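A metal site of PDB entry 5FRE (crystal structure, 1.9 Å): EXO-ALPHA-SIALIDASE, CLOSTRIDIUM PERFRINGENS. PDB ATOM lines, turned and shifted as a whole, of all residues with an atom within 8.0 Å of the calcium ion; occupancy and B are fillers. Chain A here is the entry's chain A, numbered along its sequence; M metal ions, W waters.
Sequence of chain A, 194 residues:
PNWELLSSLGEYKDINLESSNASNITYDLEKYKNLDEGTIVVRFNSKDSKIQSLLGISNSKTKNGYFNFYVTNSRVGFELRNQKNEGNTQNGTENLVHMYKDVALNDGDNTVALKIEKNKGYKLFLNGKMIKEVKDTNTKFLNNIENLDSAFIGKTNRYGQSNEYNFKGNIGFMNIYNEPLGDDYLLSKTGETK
OG of Ser 46 is in hydrogen-bond range of N of Asp 48 (3.2 Å).
The side-chain hydroxyl (OG) of Ser 46 sits at hydrogen-bond distance from the backbone carbonyl oxygen (O) of Lys 168 (3.3 Å).
The side-chain amide oxygen (OD1) of Asn 45 sits close to the backbone carbonyl oxygen (O) of Gly 108 (3.3 Å).
The backbone NH (N) of Asn 45 is in hydrogen-bond range of the backbone carbonyl oxygen (O) of Asn 170 (2.9 Å).
The calcium ion is bound by O of Ser 46.
OD1 of Asn 45 binds the calcium ion, 2.3 Å away.
O of Asp 107 binds the calcium ion (2.4 Å).
Water W3 binds the calcium ion (2.4 Å).
The calcium ion is bound by water W1 (2.4 Å).
Water W4 is bound to the calcium ion (2.5 Å).
The calcium ion is bound by water W2 (2.5 Å).
Three residues have an atom within 4 Å of the calcium ion: Asn 45, Ser 46 and Asp 107.
Along chain A the residues within 4 Å of the calcium ion span positions 45 to 107.
The nearest printed residue that does not touch the calcium ion is Lys 47 (4.4 Å).
Water W1 lies within hydrogen-bond range of O of Gly 108 (2.7 Å), O of Asn 106 (2.8 Å) and ND2 of Asn 110 (3.4 Å).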
ATOM      1  N   PHE A  44      -5.531  15.904 -15.273  1.00  0.00           N
ATOM      2  CA  PHE A  44      -4.587  15.978 -16.381  1.00  0.00           C
ATOM      3  C   PHE A  44      -5.244  16.644 -17.602  1.00  0.00           C
ATOM      4  O   PHE A  44      -6.466  16.655 -17.746  1.00  0.00           O
ATOM      5  CB  PHE A  44      -4.068  14.587 -16.727  1.00  0.00           C
ATOM      6  CG  PHE A  44      -5.098  13.674 -17.373  1.00  0.00           C
ATOM      7  CD1 PHE A  44      -5.911  12.879 -16.596  1.00  0.00           C
ATOM      8  CD2 PHE A  44      -5.242  13.622 -18.766  1.00  0.00           C
ATOM      9  CE1 PHE A  44      -6.902  12.065 -17.165  1.00  0.00           C
ATOM     10  CE2 PHE A  44      -6.211  12.802 -19.363  1.00  0.00           C
ATOM     11  CZ  PHE A  44      -7.031  11.997 -18.547  1.00  0.00           C
ATOM     12  N   ASN A  45      -4.404  17.167 -18.471  1.00  0.00           N
ATOM     13  CA  ASN A  45      -4.818  17.781 -19.748  1.00  0.00           C
ATOM     14  C   ASN A  45      -3.716  17.580 -20.766  1.00  0.00           C
ATOM     15  O   ASN A  45      -2.729  18.290 -20.772  1.00  0.00           O
ATOM     16  CB  ASN A  45      -5.160  19.280 -19.613  1.00  0.00           C
ATOM     17  CG  ASN A  45      -5.734  19.866 -20.887  1.00  0.00           C
ATOM     18  OD1 ASN A  45      -5.942  19.179 -21.906  1.00  0.00           O
ATOM     19  ND2 ASN A  45      -6.070  21.132 -20.816  1.00  0.00           N
ATOM     20  N   SER A  46      -3.914  16.582 -21.609  1.00  0.00           N
ATOM     21  CA  SER A  46      -2.992  16.234 -22.648  1.00  0.00           C
ATOM     22  C   SER A  46      -3.323  17.019 -23.913  1.00  0.00           C
ATOM     23  O   SER A  46      -4.478  17.300 -24.176  1.00  0.00           O
ATOM     24  CB  SER A  46      -3.082  14.753 -22.998  1.00  0.00           C
ATOM     25  OG  SER A  46      -2.057  14.448 -23.935  1.00  0.00           O
ATOM     26  N   LYS A  47      -2.291  17.236 -24.719  1.00  0.00           N
ATOM     27  CA  LYS A  47      -2.367  17.859 -26.032  1.00  0.00           C
ATOM     28  C   LYS A  47      -2.008  16.878 -27.170  1.00  0.00           C
ATOM     29  O   LYS A  47      -1.917  17.302 -28.299  1.00  0.00           O
ATOM     30  CB  LYS A  47      -1.366  19.035 -26.088  1.00  0.00           C
ATOM     31  N   ASP A  48      -1.799  15.586 -26.903  1.00  0.00           N
ATOM     32  CA  ASP A  48      -1.467  14.610 -27.953  1.00  0.00           C
ATOM     33  C   ASP A  48      -2.404  13.410 -27.871  1.00  0.00           C
ATOM     34  O   ASP A  48      -3.093  13.218 -26.869  1.00  0.00           O
ATOM     35  CB  ASP A  48       0.008  14.161 -27.882  1.00  0.00           C
ATOM     36  CG  ASP A  48       0.588  13.753 -29.259  1.00  0.00           C
ATOM     37  OD1 ASP A  48      -0.044  12.991 -30.032  1.00  0.00           O
ATOM     38  OD2 ASP A  48       1.682  14.199 -29.611  1.00  0.00           O
ATOM     39  N   ASN A  73      -5.880  10.222 -26.356  1.00  0.00           N
ATOM     40  CA  ASN A  73      -7.072  11.114 -26.470  1.00  0.00           C
ATOM     41  C   ASN A  73      -8.439  10.431 -26.402  1.00  0.00           C
ATOM     42  O   ASN A  73      -9.453  11.114 -26.381  1.00  0.00           O
ATOM     43  CB  ASN A  73      -7.009  11.951 -27.745  1.00  0.00           C
ATOM     44  CG  ASN A  73      -7.017  11.108 -28.989  1.00  0.00           C
ATOM     45  OD1 ASN A  73      -6.660   9.916 -28.995  1.00  0.00           O
ATOM     46  ND2 ASN A  73      -7.402  11.733 -30.081  1.00  0.00           N
ATOM     47  N   LEU A 105     -12.927  11.818 -23.886  1.00  0.00           N
ATOM     48  CA  LEU A 105     -12.229  12.708 -22.973  1.00  0.00           C
ATOM     49  C   LEU A 105     -12.608  14.188 -23.205  1.00  0.00           C
ATOM     50  O   LEU A 105     -12.969  14.559 -24.280  1.00  0.00           O
ATOM     51  CB  LEU A 105     -10.725  12.471 -23.066  1.00  0.00           C
ATOM     52  CG  LEU A 105     -10.330  11.153 -22.388  1.00  0.00           C
ATOM     53  CD1 LEU A 105      -8.977  10.693 -22.872  1.00  0.00           C
ATOM     54  CD2 LEU A 105     -10.302  11.271 -20.875  1.00  0.00           C
ATOM     55  N   ASN A 106     -12.537  15.008 -22.156  1.00  0.00           N
ATOM     56  CA  ASN A 106     -12.701  16.480 -22.315  1.00  0.00           C
ATOM     57  C   ASN A 106     -11.550  17.067 -23.071  1.00  0.00           C
ATOM     58  O   ASN A 106     -10.443  16.596 -22.917  1.00  0.00           O
ATOM     59  CB  ASN A 106     -12.717  17.198 -20.956  1.00  0.00           C
ATOM     60  CG  ASN A 106     -13.845  16.744 -20.054  1.00  0.00           C
ATOM     61  OD1 ASN A 106     -13.695  16.684 -18.813  1.00  0.00           O
ATOM     62  ND2 ASN A 106     -14.959  16.433 -20.656  1.00  0.00           N
ATOM     63  N   ASP A 107     -11.793  18.125 -23.870  1.00  0.00           N
ATOM     64  CA  ASP A 107     -10.679  18.885 -24.465  1.00  0.00           C
ATOM     65  C   ASP A 107      -9.701  19.497 -23.419  1.00  0.00           C
ATOM     66  O   ASP A 107      -8.484  19.596 -23.695  1.00  0.00           O
ATOM     67  CB  ASP A 107     -11.197  20.047 -25.360  1.00  0.00           C
ATOM     68  CG  ASP A 107     -12.024  19.549 -26.550  1.00  0.00           C
ATOM     69  OD1 ASP A 107     -11.807  18.412 -27.012  1.00  0.00           O
ATOM     70  OD2 ASP A 107     -12.897  20.315 -27.026  1.00  0.00           O
ATOM     71  N   GLY A 108     -10.234  19.966 -22.298  1.00  0.00           N
ATOM     72  CA  GLY A 108      -9.443  20.569 -21.221  1.00  0.00           C
ATOM     73  C   GLY A 108      -9.167  19.526 -20.137  1.00  0.00           C
ATOM     74  O   GLY A 108      -8.835  18.392 -20.457  1.00  0.00           O
ATOM     75  N   ASP A 109      -9.342  19.901 -18.881  1.00  0.00           N
ATOM     76  CA  ASP A 109      -9.028  19.011 -17.730  1.00  0.00           C
ATOM     77  C   ASP A 109      -9.897  17.756 -17.672  1.00  0.00           C
ATOM     78  O   ASP A 109     -11.087  17.794 -17.933  1.00  0.00           O
ATOM     79  CB  ASP A 109      -9.083  19.787 -16.413  1.00  0.00           C
ATOM     80  CG  ASP A 109      -7.827  20.653 -16.188  1.00  0.00           C
ATOM     81  OD1 ASP A 109      -6.779  20.398 -16.841  1.00  0.00           O
ATOM     82  OD2 ASP A 109      -7.865  21.588 -15.350  1.00  0.00           O
ATOM     83  N   ASN A 110      -9.257  16.626 -17.377  1.00  0.00           N
ATOM     84  CA  ASN A 110      -9.956  15.380 -17.060  1.00  0.00           C
ATOM     85  C   ASN A 110      -9.408  14.854 -15.728  1.00  0.00           C
ATOM     86  O   ASN A 110      -8.265  15.156 -15.354  1.00  0.00           O
ATOM     87  CB  ASN A 110      -9.712  14.332 -18.142  1.00  0.00           C
ATOM     88  CG  ASN A 110     -10.341  14.696 -19.465  1.00  0.00           C
ATOM     89  OD1 ASN A 110     -11.567  14.531 -19.674  1.00  0.00           O
ATOM     90  ND2 ASN A 110      -9.505  15.192 -20.396  1.00  0.00           N
ATOM     91  N   PHE A 167       4.329  12.182 -21.780  1.00  0.00           N
ATOM     92  CA  PHE A 167       3.148  12.975 -21.714  1.00  0.00           C
ATOM     93  C   PHE A 167       3.481  14.373 -22.216  1.00  0.00           C
ATOM     94  O   PHE A 167       4.556  14.915 -21.895  1.00  0.00           O
ATOM     95  CB  PHE A 167       2.682  13.072 -20.262  1.00  0.00           C
ATOM     96  CG  PHE A 167       1.328  13.686 -20.076  1.00  0.00           C
ATOM     97  CD1 PHE A 167       1.166  15.058 -19.965  1.00  0.00           C
ATOM     98  CD2 PHE A 167       0.201  12.882 -19.955  1.00  0.00           C
ATOM     99  CE1 PHE A 167      -0.081  15.612 -19.780  1.00  0.00           C
ATOM    100  CE2 PHE A 167      -1.077  13.438 -19.783  1.00  0.00           C
ATOM    101  CZ  PHE A 167      -1.209  14.809 -19.659  1.00  0.00           C
ATOM    102  N   LYS A 168       2.547  14.931 -22.954  1.00  0.00           N
ATOM    103  CA  LYS A 168       2.605  16.328 -23.383  1.00  0.00           C
ATOM    104  C   LYS A 168       1.341  17.046 -22.955  1.00  0.00           C
ATOM    105  O   LYS A 168       0.221  16.706 -23.388  1.00  0.00           O
ATOM    106  CB  LYS A 168       2.782  16.446 -24.911  1.00  0.00           C
ATOM    107  CG  LYS A 168       2.980  17.900 -25.356  1.00  0.00           C
ATOM    108  CD  LYS A 168       3.930  18.060 -26.523  1.00  0.00           C
ATOM    109  CE  LYS A 168       4.264  19.528 -26.772  1.00  0.00           C
ATOM    110  NZ  LYS A 168       5.742  19.683 -26.659  1.00  0.00           N
ATOM    111  N   GLY A 169       1.517  18.019 -22.084  1.00  0.00           N
ATOM    112  CA  GLY A 169       0.434  18.838 -21.595  1.00  0.00           C
ATOM    113  C   GLY A 169       0.750  19.252 -20.178  1.00  0.00           C
ATOM    114  O   GLY A 169       1.903  19.597 -19.863  1.00  0.00           O
ATOM    115  N   ASN A 170      -0.273  19.252 -19.307  1.00  0.00           N
ATOM    116  CA  ASN A 170      -0.038  19.472 -17.901  1.00  0.00           C
ATOM    117  C   ASN A 170      -0.821  18.499 -16.985  1.00  0.00           C
ATOM    118  O   ASN A 170      -1.891  18.021 -17.344  1.00  0.00           O
ATOM    119  CB  ASN A 170      -0.280  20.931 -17.516  1.00  0.00           C
ATOM    120  CG  ASN A 170      -1.729  21.237 -17.285  1.00  0.00           C
ATOM    121  OD1 ASN A 170      -2.208  21.185 -16.149  1.00  0.00           O
ATOM    122  ND2 ASN A 170      -2.449  21.565 -18.348  1.00  0.00           N
HETATM  123 CA    CA M   1      -6.411  18.523 -24.098  1.00  0.00          CA
HETATM  124  O   HOH W   1      -7.732  17.146 -22.570  1.00  0.00           O
HETATM  125  O   HOH W   2      -5.816  19.465 -26.311  1.00  0.00           O
HETATM  126  O   HOH W   3      -5.172  20.562 -24.375  1.00  0.00           O
HETATM  127  O   HOH W   4      -7.463  16.934 -25.654  1.00  0.00           O
